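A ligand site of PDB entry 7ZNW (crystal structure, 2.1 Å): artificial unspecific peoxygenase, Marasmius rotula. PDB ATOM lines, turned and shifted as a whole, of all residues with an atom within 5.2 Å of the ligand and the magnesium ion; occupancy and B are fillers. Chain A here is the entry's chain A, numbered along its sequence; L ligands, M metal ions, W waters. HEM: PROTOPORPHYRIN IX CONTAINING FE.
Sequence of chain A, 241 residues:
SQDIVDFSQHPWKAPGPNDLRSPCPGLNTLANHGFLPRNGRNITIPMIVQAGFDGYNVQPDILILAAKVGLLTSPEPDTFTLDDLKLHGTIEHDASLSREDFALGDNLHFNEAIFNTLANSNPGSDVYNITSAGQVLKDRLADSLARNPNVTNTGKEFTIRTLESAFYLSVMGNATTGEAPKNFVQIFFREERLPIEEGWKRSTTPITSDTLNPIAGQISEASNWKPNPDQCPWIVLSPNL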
ATOM      1  N   PRO A  23      13.763 -28.936  -1.151  1.00  0.00           N
ATOM      2  CA  PRO A  23      12.384 -29.407  -1.201  1.00  0.00           C
ATOM      3  C   PRO A  23      11.862 -29.563  -2.647  1.00  0.00           C
ATOM      4  O   PRO A  23      10.668 -29.800  -2.801  1.00  0.00           O
ATOM      5  CB  PRO A  23      11.592 -28.304  -0.475  1.00  0.00           C
ATOM      6  CG  PRO A  23      12.615 -27.270  -0.033  1.00  0.00           C
ATOM      7  CD  PRO A  23      13.833 -27.497  -0.896  1.00  0.00           C
ATOM      8  N   CYS A  24      12.749 -29.426  -3.630  1.00  0.00           N
ATOM      9  CA  CYS A  24      12.363 -29.447  -5.060  1.00  0.00           C
ATOM     10  C   CYS A  24      12.796 -30.758  -5.725  1.00  0.00           C
ATOM     11  O   CYS A  24      14.000 -30.914  -5.952  1.00  0.00           O
ATOM     12  CB  CYS A  24      12.984 -28.288  -5.824  1.00  0.00           C
ATOM     13  SG  CYS A  24      12.655 -28.353  -7.594  1.00  0.00           S
ATOM     14  N   PRO A  25      11.869 -31.658  -6.113  1.00  0.00           N
ATOM     15  CA  PRO A  25      12.249 -32.864  -6.834  1.00  0.00           C
ATOM     16  C   PRO A  25      12.933 -32.522  -8.154  1.00  0.00           C
ATOM     17  O   PRO A  25      13.745 -33.297  -8.590  1.00  0.00           O
ATOM     18  CB  PRO A  25      10.912 -33.609  -7.045  1.00  0.00           C
ATOM     19  CG  PRO A  25       9.867 -32.503  -6.963  1.00  0.00           C
ATOM     20  CD  PRO A  25      10.420 -31.570  -5.910  1.00  0.00           C
ATOM     21  N   GLY A  26      12.598 -31.372  -8.772  1.00  0.00           N
ATOM     22  CA  GLY A  26      13.212 -30.980 -10.053  1.00  0.00           C
ATOM     23  C   GLY A  26      14.716 -30.837  -9.934  1.00  0.00           C
ATOM     24  O   GLY A  26      15.451 -31.523 -10.661  1.00  0.00           O
ATOM     25  N   LEU A  27      15.185 -30.005  -8.999  1.00  0.00           N
ATOM     26  CA  LEU A  27      16.621 -29.764  -8.790  1.00  0.00           C
ATOM     27  C   LEU A  27      17.275 -30.991  -8.175  1.00  0.00           C
ATOM     28  O   LEU A  27      18.403 -31.309  -8.592  1.00  0.00           O
ATOM     29  CB  LEU A  27      16.804 -28.525  -7.907  1.00  0.00           C
ATOM     30  CG  LEU A  27      16.228 -27.221  -8.471  1.00  0.00           C
ATOM     31  CD1 LEU A  27      16.628 -26.050  -7.570  1.00  0.00           C
ATOM     32  CD2 LEU A  27      16.667 -26.992  -9.912  1.00  0.00           C
ATOM     33  N   LEU A  30      18.026 -33.463 -10.846  1.00  0.00           N
ATOM     34  CA  LEU A  30      19.178 -32.950 -11.652  1.00  0.00           C
ATOM     35  C   LEU A  30      20.493 -33.198 -10.877  1.00  0.00           C
ATOM     36  O   LEU A  30      21.445 -33.675 -11.507  1.00  0.00           O
ATOM     37  CB  LEU A  30      18.970 -31.474 -11.969  1.00  0.00           C
ATOM     38  CG  LEU A  30      17.874 -31.159 -12.996  1.00  0.00           C
ATOM     39  CD1 LEU A  30      17.656 -29.662 -13.150  1.00  0.00           C
ATOM     40  CD2 LEU A  30      18.194 -31.773 -14.341  1.00  0.00           C
ATOM     41  N   ILE A  48      21.980 -23.544 -13.082  1.00  0.00           N
ATOM     42  CA  ILE A  48      20.524 -23.891 -13.075  1.00  0.00           C
ATOM     43  C   ILE A  48      19.970 -23.911 -14.524  1.00  0.00           C
ATOM     44  O   ILE A  48      19.290 -24.882 -14.851  1.00  0.00           O
ATOM     45  CB  ILE A  48      19.706 -22.963 -12.155  1.00  0.00           C
ATOM     46  CG1 ILE A  48      20.125 -23.165 -10.696  1.00  0.00           C
ATOM     47  CG2 ILE A  48      18.213 -23.188 -12.349  1.00  0.00           C
ATOM     48  CD1 ILE A  48      19.562 -24.436 -10.055  1.00  0.00           C
ATOM     49  N   GLY A  52      18.685 -27.389 -16.239  1.00  0.00           N
ATOM     50  CA  GLY A  52      17.256 -27.432 -16.598  1.00  0.00           C
ATOM     51  C   GLY A  52      17.054 -27.726 -18.082  1.00  0.00           C
ATOM     52  O   GLY A  52      16.165 -28.557 -18.428  1.00  0.00           O
ATOM     53  N   TYR A  56      15.738 -31.574 -18.838  1.00  0.00           N
ATOM     54  CA  TYR A  56      14.269 -31.537 -18.988  1.00  0.00           C
ATOM     55  C   TYR A  56      13.836 -30.789 -20.264  1.00  0.00           C
ATOM     56  O   TYR A  56      12.608 -30.795 -20.555  1.00  0.00           O
ATOM     57  CB  TYR A  56      13.620 -30.841 -17.789  1.00  0.00           C
ATOM     58  CG  TYR A  56      13.891 -31.420 -16.424  1.00  0.00           C
ATOM     59  CD1 TYR A  56      13.719 -32.772 -16.168  1.00  0.00           C
ATOM     60  CD2 TYR A  56      14.258 -30.598 -15.361  1.00  0.00           C
ATOM     61  CE1 TYR A  56      13.907 -33.298 -14.891  1.00  0.00           C
ATOM     62  CE2 TYR A  56      14.441 -31.112 -14.079  1.00  0.00           C
ATOM     63  CZ  TYR A  56      14.270 -32.463 -13.845  1.00  0.00           C
ATOM     64  OH  TYR A  56      14.453 -32.994 -12.600  1.00  0.00           O
ATOM     65  N   VAL A  58      13.836 -27.606 -20.283  1.00  0.00           N
ATOM     66  CA  VAL A  58      13.190 -26.365 -19.765  1.00  0.00           C
ATOM     67  C   VAL A  58      14.052 -25.159 -20.211  1.00  0.00           C
ATOM     68  O   VAL A  58      15.293 -25.201 -20.034  1.00  0.00           O
ATOM     69  CB  VAL A  58      12.949 -26.418 -18.248  1.00  0.00           C
ATOM     70  CG1 VAL A  58      12.425 -25.088 -17.739  1.00  0.00           C
ATOM     71  CG2 VAL A  58      11.977 -27.521 -17.878  1.00  0.00           C
ATOM     72  N   LEU A  63      13.529 -20.545 -15.479  1.00  0.00           N
ATOM     73  CA  LEU A  63      14.652 -20.953 -14.581  1.00  0.00           C
ATOM     74  C   LEU A  63      15.403 -19.752 -13.993  1.00  0.00           C
ATOM     75  O   LEU A  63      15.809 -19.803 -12.796  1.00  0.00           O
ATOM     76  CB  LEU A  63      15.599 -21.870 -15.354  1.00  0.00           C
ATOM     77  CG  LEU A  63      14.963 -23.192 -15.794  1.00  0.00           C
ATOM     78  CD1 LEU A  63      15.895 -23.967 -16.707  1.00  0.00           C
ATOM     79  CD2 LEU A  63      14.579 -24.028 -14.587  1.00  0.00           C
ATOM     80  N   ALA A  66      13.246 -18.180 -11.152  1.00  0.00           N
ATOM     81  CA  ALA A  66      13.171 -19.066  -9.983  1.00  0.00           C
ATOM     82  C   ALA A  66      14.535 -19.031  -9.269  1.00  0.00           C
ATOM     83  O   ALA A  66      14.582 -18.952  -8.041  1.00  0.00           O
ATOM     84  CB  ALA A  66      12.753 -20.469 -10.396  1.00  0.00           C
ATOM     85  N   ALA A  67      15.620 -19.099 -10.024  1.00  0.00           N
ATOM     86  CA  ALA A  67      16.981 -19.156  -9.459  1.00  0.00           C
ATOM     87  C   ALA A  67      17.331 -17.827  -8.780  1.00  0.00           C
ATOM     88  O   ALA A  67      17.993 -17.831  -7.721  1.00  0.00           O
ATOM     89  CB  ALA A  67      17.974 -19.517 -10.532  1.00  0.00           C
ATOM     90  N   GLY A  70      15.608 -17.962  -5.563  1.00  0.00           N
ATOM     91  CA  GLY A  70      16.358 -18.979  -4.792  1.00  0.00           C
ATOM     92  C   GLY A  70      17.609 -18.388  -4.160  1.00  0.00           C
ATOM     93  O   GLY A  70      17.919 -18.734  -2.972  1.00  0.00           O
ATOM     94  N   PHE A  80      23.920 -20.550  -4.246  1.00  0.00           N
ATOM     95  CA  PHE A  80      23.103 -21.168  -3.170  1.00  0.00           C
ATOM     96  C   PHE A  80      23.414 -22.660  -3.185  1.00  0.00           C
ATOM     97  O   PHE A  80      23.936 -23.195  -4.189  1.00  0.00           O
ATOM     98  CB  PHE A  80      21.612 -20.872  -3.324  1.00  0.00           C
ATOM     99  CG  PHE A  80      20.986 -21.311  -4.632  1.00  0.00           C
ATOM    100  CD1 PHE A  80      20.624 -22.630  -4.853  1.00  0.00           C
ATOM    101  CD2 PHE A  80      20.693 -20.376  -5.618  1.00  0.00           C
ATOM    102  CE1 PHE A  80      20.030 -23.014  -6.052  1.00  0.00           C
ATOM    103  CE2 PHE A  80      20.081 -20.755  -6.809  1.00  0.00           C
ATOM    104  CZ  PHE A  80      19.764 -22.078  -7.027  1.00  0.00           C
ATOM    105  N   LEU A  85      17.407 -23.626  -0.136  1.00  0.00           N
ATOM    106  CA  LEU A  85      16.091 -23.385  -0.812  1.00  0.00           C
ATOM    107  C   LEU A  85      14.915 -23.744   0.122  1.00  0.00           C
ATOM    108  O   LEU A  85      13.786 -23.368  -0.208  1.00  0.00           O
ATOM    109  CB  LEU A  85      16.046 -24.226  -2.099  1.00  0.00           C
ATOM    110  CG  LEU A  85      17.082 -23.847  -3.149  1.00  0.00           C
ATOM    111  CD1 LEU A  85      16.982 -24.794  -4.346  1.00  0.00           C
ATOM    112  CD2 LEU A  85      16.943 -22.387  -3.552  1.00  0.00           C
ATOM    113  N   ILE A  91      10.475 -19.244  -1.672  1.00  0.00           N
ATOM    114  CA  ILE A  91       9.685 -20.147  -2.568  1.00  0.00           C
ATOM    115  C   ILE A  91       8.943 -21.170  -1.704  1.00  0.00           C
ATOM    116  O   ILE A  91       7.721 -21.322  -1.895  1.00  0.00           O
ATOM    117  CB  ILE A  91      10.616 -20.818  -3.591  1.00  0.00           C
ATOM    118  CG1 ILE A  91      11.279 -19.787  -4.509  1.00  0.00           C
ATOM    119  CG2 ILE A  91       9.871 -21.868  -4.403  1.00  0.00           C
ATOM    120  CD1 ILE A  91      12.421 -20.341  -5.320  1.00  0.00           C
ATOM    121  N   GLU A  92       9.654 -21.841  -0.779  1.00  0.00           N
ATOM    122  CA  GLU A  92       9.077 -22.962   0.008  1.00  0.00           C
ATOM    123  C   GLU A  92       7.785 -22.444   0.664  1.00  0.00           C
ATOM    124  O   GLU A  92       7.756 -21.312   1.204  1.00  0.00           O
ATOM    125  CB  GLU A  92      10.100 -23.545   0.988  1.00  0.00           C
ATOM    126  CG  GLU A  92       9.624 -24.860   1.573  1.00  0.00           C
ATOM    127  CD  GLU A  92       8.530 -24.707   2.623  1.00  0.00           C
ATOM    128  OE1 GLU A  92       8.584 -23.700   3.368  1.00  0.00           O
ATOM    129  OE2 GLU A  92       7.624 -25.566   2.697  1.00  0.00           O
ATOM    130  N   HIS A  93       6.722 -23.236   0.507  1.00  0.00           N
ATOM    131  CA  HIS A  93       5.336 -22.846   0.890  1.00  0.00           C
ATOM    132  C   HIS A  93       4.633 -24.024   1.563  1.00  0.00           C
ATOM    133  O   HIS A  93       5.023 -25.200   1.360  1.00  0.00           O
ATOM    134  CB  HIS A  93       4.574 -22.366  -0.350  1.00  0.00           C
ATOM    135  CG  HIS A  93       4.592 -23.400  -1.437  1.00  0.00           C
ATOM    136  ND1 HIS A  93       3.885 -24.605  -1.340  1.00  0.00           N
ATOM    137  CD2 HIS A  93       5.287 -23.463  -2.592  1.00  0.00           C
ATOM    138  CE1 HIS A  93       4.135 -25.346  -2.397  1.00  0.00           C
ATOM    139  NE2 HIS A  93       5.007 -24.662  -3.196  1.00  0.00           N
ATOM    140  N   ASP A  94       3.581 -23.703   2.311  1.00  0.00           N
ATOM    141  CA  ASP A  94       2.612 -24.664   2.873  1.00  0.00           C
ATOM    142  C   ASP A  94       1.872 -25.385   1.731  1.00  0.00           C
ATOM    143  O   ASP A  94       1.861 -24.842   0.604  1.00  0.00           O
ATOM    144  CB  ASP A  94       1.673 -23.923   3.838  1.00  0.00           C
ATOM    145  CG  ASP A  94       2.445 -23.296   4.981  1.00  0.00           C
ATOM    146  OD1 ASP A  94       3.537 -23.850   5.312  1.00  0.00           O
ATOM    147  OD2 ASP A  94       1.989 -22.240   5.505  1.00  0.00           O
ATOM    148  N   SER A  96       2.537 -28.263   0.166  1.00  0.00           N
ATOM    149  CA  SER A  96       3.425 -28.946  -0.798  1.00  0.00           C
ATOM    150  C   SER A  96       2.790 -30.310  -1.115  1.00  0.00           C
ATOM    151  O   SER A  96       1.992 -30.798  -0.295  1.00  0.00           O
ATOM    152  CB  SER A  96       4.847 -29.113  -0.281  1.00  0.00           C
ATOM    153  OG  SER A  96       5.480 -27.868  -0.043  1.00  0.00           O
ATOM    154  N   LEU A  97       3.189 -30.893  -2.233  1.00  0.00           N
ATOM    155  CA  LEU A  97       2.716 -32.199  -2.725  1.00  0.00           C
ATOM    156  C   LEU A  97       3.350 -33.348  -1.955  1.00  0.00           C
ATOM    157  O   LEU A  97       2.721 -34.417  -1.894  1.00  0.00           O
ATOM    158  CB  LEU A  97       3.071 -32.288  -4.207  1.00  0.00           C
ATOM    159  CG  LEU A  97       2.478 -31.205  -5.096  1.00  0.00           C
ATOM    160  CD1 LEU A  97       3.094 -31.268  -6.471  1.00  0.00           C
ATOM    161  CD2 LEU A  97       0.960 -31.346  -5.197  1.00  0.00           C
ATOM    162  N   SER A  98       4.589 -33.192  -1.484  1.00  0.00           N
ATOM    163  CA  SER A  98       5.397 -34.325  -0.935  1.00  0.00           C
ATOM    164  C   SER A  98       6.175 -33.930   0.334  1.00  0.00           C
ATOM    165  O   SER A  98       6.946 -34.773   0.803  1.00  0.00           O
ATOM    166  CB  SER A  98       6.332 -34.837  -1.994  1.00  0.00           C
ATOM    167  OG  SER A  98       7.286 -33.847  -2.335  1.00  0.00           O
ATOM    168  N   ARG A  99       5.922 -32.737   0.847  1.00  0.00           N
ATOM    169  CA  ARG A  99       6.620 -32.261   2.066  1.00  0.00           C
ATOM    170  C   ARG A  99       5.618 -31.725   3.091  1.00  0.00           C
ATOM    171  O   ARG A  99       4.585 -31.203   2.664  1.00  0.00           O
ATOM    172  CB  ARG A  99       7.639 -31.172   1.686  1.00  0.00           C
ATOM    173  CG  ARG A  99       9.061 -31.679   1.451  1.00  0.00           C
ATOM    174  CD  ARG A  99       9.216 -32.413   0.138  1.00  0.00           C
ATOM    175  NE  ARG A  99      10.606 -32.594  -0.236  1.00  0.00           N
ATOM    176  CZ  ARG A  99      11.022 -33.349  -1.242  1.00  0.00           C
ATOM    177  NH1 ARG A  99      10.147 -33.996  -1.985  1.00  0.00           N
ATOM    178  NH2 ARG A  99      12.307 -33.444  -1.501  1.00  0.00           N
ATOM    179  N   GLU A 100       5.903 -31.882   4.383  1.00  0.00           N
ATOM    180  CA  GLU A 100       5.096 -31.286   5.473  1.00  0.00           C
ATOM    181  C   GLU A 100       5.251 -29.766   5.423  1.00  0.00           C
ATOM    182  O   GLU A 100       6.292 -29.252   4.916  1.00  0.00           O
ATOM    183  CB  GLU A 100       5.507 -31.805   6.859  1.00  0.00           C
ATOM    184  CG  GLU A 100       5.458 -33.321   6.964  1.00  0.00           C
ATOM    185  CD  GLU A 100       5.983 -33.891   8.282  1.00  0.00           C
ATOM    186  OE1 GLU A 100       6.983 -33.363   8.850  1.00  0.00           O
ATOM    187  OE2 GLU A 100       5.394 -34.867   8.741  1.00  0.00           O
ATOM    188  N   ASN A 107       9.771 -29.387   6.270  1.00  0.00           N
ATOM    189  CA  ASN A 107       9.413 -28.796   4.955  1.00  0.00           C
ATOM    190  C   ASN A 107      10.481 -29.108   3.893  1.00  0.00           C
ATOM    191  O   ASN A 107      10.407 -28.525   2.778  1.00  0.00           O
ATOM    192  CB  ASN A 107       9.196 -27.281   5.111  1.00  0.00           C
ATOM    193  CG  ASN A 107      10.479 -26.481   5.223  1.00  0.00           C
ATOM    194  OD1 ASN A 107      11.554 -26.994   5.515  1.00  0.00           O
ATOM    195  ND2 ASN A 107      10.385 -25.184   4.989  1.00  0.00           N
ATOM    196  N   GLU A 164       4.391 -25.390 -10.009  1.00  0.00           N
ATOM    197  CA  GLU A 164       5.138 -26.599  -9.594  1.00  0.00           C
ATOM    198  C   GLU A 164       4.395 -27.841 -10.094  1.00  0.00           C
ATOM    199  O   GLU A 164       5.059 -28.789 -10.549  1.00  0.00           O
ATOM    200  CB  GLU A 164       5.382 -26.572  -8.083  1.00  0.00           C
ATOM    201  CG  GLU A 164       6.349 -25.466  -7.658  1.00  0.00           C
ATOM    202  CD  GLU A 164       6.419 -25.216  -6.163  1.00  0.00           C
ATOM    203  OE1 GLU A 164       5.462 -25.639  -5.407  1.00  0.00           O
ATOM    204  OE2 GLU A 164       7.467 -24.642  -5.715  1.00  0.00           O
ATOM    205  N   SER A 165       3.057 -27.807 -10.058  1.00  0.00           N
ATOM    206  CA  SER A 165       2.186 -28.916 -10.544  1.00  0.00           C
ATOM    207  C   SER A 165       2.273 -28.981 -12.078  1.00  0.00           C
ATOM    208  O   SER A 165       2.396 -30.100 -12.621  1.00  0.00           O
ATOM    209  CB  SER A 165       0.798 -28.787 -10.038  1.00  0.00           C
ATOM    210  OG  SER A 165       0.738 -29.260  -8.714  1.00  0.00           O
ATOM    211  N   PHE A 167       4.901 -28.186 -13.616  1.00  0.00           N
ATOM    212  CA  PHE A 167       6.270 -28.699 -13.840  1.00  0.00           C
ATOM    213  C   PHE A 167       6.272 -30.233 -13.836  1.00  0.00           C
ATOM    214  O   PHE A 167       6.832 -30.805 -14.787  1.00  0.00           O
ATOM    215  CB  PHE A 167       7.270 -28.154 -12.818  1.00  0.00           C
ATOM    216  CG  PHE A 167       8.133 -27.027 -13.336  1.00  0.00           C
ATOM    217  CD1 PHE A 167       8.738 -27.108 -14.579  1.00  0.00           C
ATOM    218  CD2 PHE A 167       8.352 -25.907 -12.548  1.00  0.00           C
ATOM    219  CE1 PHE A 167       9.569 -26.092 -15.029  1.00  0.00           C
ATOM    220  CE2 PHE A 167       9.189 -24.903 -13.003  1.00  0.00           C
ATOM    221  CZ  PHE A 167       9.770 -24.987 -14.247  1.00  0.00           C
ATOM    222  N   TYR A 168       5.695 -30.888 -12.833  1.00  0.00           N
ATOM    223  CA  TYR A 168       5.765 -32.374 -12.759  1.00  0.00           C
ATOM    224  C   TYR A 168       5.027 -32.976 -13.966  1.00  0.00           C
ATOM    225  O   TYR A 168       5.560 -33.909 -14.617  1.00  0.00           O
ATOM    226  CB  TYR A 168       5.341 -32.907 -11.376  1.00  0.00           C
ATOM    227  CG  TYR A 168       3.887 -33.039 -11.028  1.00  0.00           C
ATOM    228  CD1 TYR A 168       3.057 -33.974 -11.628  1.00  0.00           C
ATOM    229  CD2 TYR A 168       3.345 -32.268 -10.011  1.00  0.00           C
ATOM    230  CE1 TYR A 168       1.722 -34.113 -11.264  1.00  0.00           C
ATOM    231  CE2 TYR A 168       2.020 -32.401  -9.628  1.00  0.00           C
ATOM    232  CZ  TYR A 168       1.198 -33.313 -10.271  1.00  0.00           C
ATOM    233  OH  TYR A 168      -0.101 -33.424  -9.872  1.00  0.00           O
ATOM    234  N   VAL A 171       7.511 -32.030 -17.273  1.00  0.00           N
ATOM    235  CA  VAL A 171       8.879 -32.586 -17.473  1.00  0.00           C
ATOM    236  C   VAL A 171       8.809 -34.115 -17.504  1.00  0.00           C
ATOM    237  O   VAL A 171       9.651 -34.711 -18.201  1.00  0.00           O
ATOM    238  CB  VAL A 171       9.914 -32.075 -16.428  1.00  0.00           C
ATOM    239  CG1 VAL A 171       9.963 -30.551 -16.367  1.00  0.00           C
ATOM    240  CG2 VAL A 171       9.691 -32.659 -15.049  1.00  0.00           C
ATOM    241  N   PHE A 188      10.012 -39.902 -10.011  1.00  0.00           N
ATOM    242  CA  PHE A 188      10.491 -38.507  -9.877  1.00  0.00           C
ATOM    243  C   PHE A 188      10.427 -38.077  -8.410  1.00  0.00           C
ATOM    244  O   PHE A 188      11.443 -37.679  -7.853  1.00  0.00           O
ATOM    245  CB  PHE A 188       9.647 -37.617 -10.801  1.00  0.00           C
ATOM    246  CG  PHE A 188      10.008 -36.160 -10.859  1.00  0.00           C
ATOM    247  CD1 PHE A 188      11.232 -35.747 -11.330  1.00  0.00           C
ATOM    248  CD2 PHE A 188       9.061 -35.199 -10.528  1.00  0.00           C
ATOM    249  CE1 PHE A 188      11.548 -34.391 -11.401  1.00  0.00           C
ATOM    250  CE2 PHE A 188       9.376 -33.851 -10.623  1.00  0.00           C
ATOM    251  CZ  PHE A 188      10.612 -33.455 -11.058  1.00  0.00           C
ATOM    252  N   PHE A 189       9.271 -38.220  -7.758  1.00  0.00           N
ATOM    253  CA  PHE A 189       9.086 -37.736  -6.363  1.00  0.00           C
ATOM    254  C   PHE A 189       9.774 -38.667  -5.361  1.00  0.00           C
ATOM    255  O   PHE A 189      10.448 -38.171  -4.447  1.00  0.00           O
ATOM    256  CB  PHE A 189       7.596 -37.551  -6.035  1.00  0.00           C
ATOM    257  CG  PHE A 189       6.993 -36.240  -6.444  1.00  0.00           C
ATOM    258  CD1 PHE A 189       7.001 -35.155  -5.576  1.00  0.00           C
ATOM    259  CD2 PHE A 189       6.389 -36.092  -7.684  1.00  0.00           C
ATOM    260  CE1 PHE A 189       6.441 -33.954  -5.948  1.00  0.00           C
ATOM    261  CE2 PHE A 189       5.814 -34.877  -8.047  1.00  0.00           C
ATOM    262  CZ  PHE A 189       5.849 -33.811  -7.183  1.00  0.00           C
HETATM  263  CHA HEM L   1       9.129 -27.326  -5.371  1.00  0.00           C
HETATM  264  CHB HEM L   1       9.688 -29.041  -9.854  1.00  0.00           C
HETATM  265  CHC HEM L   1      13.134 -25.728 -10.727  1.00  0.00           C
HETATM  266  CHD HEM L   1      12.894 -24.439  -6.088  1.00  0.00           C
HETATM  267  C1A HEM L   1       8.934 -27.992  -6.571  1.00  0.00           C
HETATM  268  C2A HEM L   1       7.876 -28.928  -6.781  1.00  0.00           C
HETATM  269  C3A HEM L   1       8.030 -29.402  -8.051  1.00  0.00           C
HETATM  270  C4A HEM L   1       9.192 -28.807  -8.592  1.00  0.00           C
HETATM  271  CMA HEM L   1       7.113 -30.398  -8.727  1.00  0.00           C
HETATM  272  CAA HEM L   1       6.753 -29.283  -5.834  1.00  0.00           C
HETATM  273  CBA HEM L   1       7.245 -30.218  -4.687  1.00  0.00           C
HETATM  274  CGA HEM L   1       6.179 -30.440  -3.648  1.00  0.00           C
HETATM  275  O1A HEM L   1       6.239 -31.443  -2.877  1.00  0.00           O
HETATM  276  O2A HEM L   1       5.239 -29.598  -3.575  1.00  0.00           O
HETATM  277  C1B HEM L   1      10.695 -28.290 -10.430  1.00  0.00           C
HETATM  278  C2B HEM L   1      11.097 -28.521 -11.775  1.00  0.00           C
HETATM  279  C3B HEM L   1      12.035 -27.592 -12.067  1.00  0.00           C
HETATM  280  C4B HEM L   1      12.228 -26.793 -10.827  1.00  0.00           C
HETATM  281  CMB HEM L   1      10.594 -29.613 -12.727  1.00  0.00           C
HETATM  282  CAB HEM L   1      12.804 -27.566 -13.311  1.00  0.00           C
HETATM  283  CBB HEM L   1      14.122 -27.233 -13.264  1.00  0.00           C
HETATM  284  C1C HEM L   1      13.362 -25.038  -9.569  1.00  0.00           C
HETATM  285  C2C HEM L   1      14.244 -23.981  -9.394  1.00  0.00           C
HETATM  286  C3C HEM L   1      14.189 -23.629  -8.035  1.00  0.00           C
HETATM  287  C4C HEM L   1      13.250 -24.477  -7.429  1.00  0.00           C
HETATM  288  CMC HEM L   1      15.139 -23.400 -10.454  1.00  0.00           C
HETATM  289  CAC HEM L   1      14.956 -22.635  -7.265  1.00  0.00           C
HETATM  290  CBC HEM L   1      16.109 -22.203  -7.703  1.00  0.00           C
HETATM  291  C1D HEM L   1      11.853 -25.156  -5.534  1.00  0.00           C
HETATM  292  C2D HEM L   1      11.483 -24.974  -4.115  1.00  0.00           C
HETATM  293  C3D HEM L   1      10.422 -25.785  -3.891  1.00  0.00           C
HETATM  294  C4D HEM L   1      10.170 -26.424  -5.205  1.00  0.00           C
HETATM  295  CMD HEM L   1      12.150 -24.054  -3.077  1.00  0.00           C
HETATM  296  CAD HEM L   1       9.675 -25.920  -2.557  1.00  0.00           C
HETATM  297  CBD HEM L   1       8.231 -25.429  -2.702  1.00  0.00           C
HETATM  298  CGD HEM L   1       7.286 -26.162  -1.785  1.00  0.00           C
HETATM  299  O1D HEM L   1       6.974 -25.592  -0.715  1.00  0.00           O
HETATM  300  O2D HEM L   1       6.821 -27.309  -2.060  1.00  0.00           O
HETATM  301  NA  HEM L   1       9.736 -27.922  -7.698  1.00  0.00           N
HETATM  302  NB  HEM L   1      11.387 -27.285  -9.925  1.00  0.00           N
HETATM  303  NC  HEM L   1      12.756 -25.318  -8.410  1.00  0.00           N
HETATM  304  ND  HEM L   1      11.036 -26.021  -6.147  1.00  0.00           N
HETATM  305 FE   HEM L   1      11.177 -26.583  -7.980  1.00  0.00          FE
HETATM  306 MG    MG M   1       6.572 -26.656   1.199  1.00  0.00          MG
HETATM  307  O   HOH W   1       3.909 -27.631  -4.784  1.00  0.00           O
HETATM  308  O   HOH W   2       8.591 -29.273  -1.151  1.00  0.00           O
HETATM  309  O   HOH W   3       8.213 -27.896   1.011  1.00  0.00           O
HETATM  310  O   HOH W   4       5.628 -27.752   2.724  1.00  0.00           O
HETATM  311  O   HOH W   5       9.681 -25.076  -8.567  1.00  0.00           O
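Water W3 lies within hydrogen-bond range of the backbone carbonyl oxygen of Asn 107 (2.9 Å) and an oxygen (O2D) of the ligand (3.4 Å). Water W1 bridges OE1 of Glu 164 (2.6 Å) and O2A of the ligand (2.7 Å). Water W2 bridges O of Pro 23 (2.7 Å) and O2D of the ligand (2.8 Å).
The backbone NH (N) of Ser 98 lies within hydrogen-bond range of an oxygen (O1A) of the ligand (2.8 Å). The side-chain sulfur of Cys 24 binds an iron atom (FE) of the ligand, at 2.3 Å. An oxygen (O1D) of the ligand sits close to the backbone NH (N) of His 93. An oxygen (O2A) of the ligand sits at hydrogen-bond distance from the backbone NH of Leu 97, 2.8 Å away. An oxygen (O2D) of the ligand lies close to a ring nitrogen (NE2) of His 93, at 3.4 Å. OG of Ser 98 lies within hydrogen-bond range of O1A of the ligand, 2.7 Å away.
The magnesium ion is bound by OG of Ser 96 (2.1 Å). Water W3 is bound to the magnesium ion (2.1 Å). Water W4 is bound to the magnesium ion (2.1 Å). OE2 of Glu 92 binds the magnesium ion (2.1 Å). The magnesium ion is bound by O of His 93 (2.1 Å). The magnesium ion is bound by O1D of the ligand (2.2 Å).
Pro 23 touches the ligand. Pro 25 touches the ligand. Gly 26 touches the ligand (CA to C2B, 3.7 Å). Leu 27 touches the ligand (CD1 to C3C, 3.5 Å). CG2 of Ile 48 touches CMC of the ligand (3.6 Å). Tyr 56 touches the ligand. Leu 63 touches the ligand (CD2 to CBB, 3.5 Å). Ala 66 touches the ligand (O to CBC, 3.6 Å). Ala 67 touches the ligand. Phe 80 touches the ligand. Leu 85 touches the ligand (O to CMD, 3.4 Å). CG2 of Ile 91 touches CMD of the ligand (3.4 Å). Arg 99 touches the ligand. Glu 164 touches the ligand (OE2 to CHA, 3.2 Å). CG of Phe 167 touches CMB of the ligand, at 3.6 Å. CG1 of Val 171 touches CMB of the ligand, at 3.8 Å. Phe 189 touches the ligand (CZ to CMA, 3.95 Å). Hydrophobic or aromatic side chains that line the ligand: Pro 23, Pro 25, Leu 27, Ile 48, Tyr 56, Leu 63, Ala 66, Phe 80, Ile 91, His 93, Leu 97, Phe 167, Val 171 and Phe 189. Within 4 Å of the ligand: Pro 23, Cys 24, Pro 25, Gly 26, Leu 27, Ile 48, Tyr 56, Leu 63, Ala 66, Ala 67, Phe 80, Leu 85, Ile 91, Glu 92, His 93, Ser 96, Leu 97, Ser 98, Arg 99, Glu 164, Phe 167, Val 171 and Phe 189.
The side-chain sulfur (SG) of Cys 24 lies close to the backbone NH (N) of Leu 27 (3.3 Å). The side-chain carboxylate (OE1) of Glu 92 sits at hydrogen-bond distance from the side-chain amide nitrogen (ND2) of Asn 107 (2.8 Å). The side-chain hydroxyl of Tyr 56 lies within hydrogen-bond range of the backbone carbonyl oxygen of Gly 26, 2.6 Å away. OE1 of Glu 164 sits at hydrogen-bond distance from NE2 of His 93. N of Gly 26 sits close to SG of Cys 24. The side-chain hydroxyl (OG) of Ser 98 lies within hydrogen-bond range of the guanidinium group (NH1) of Arg 99 (2.9 Å).
Of the 33 residues printed, 3 come within 4 Å of the magnesium ion.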
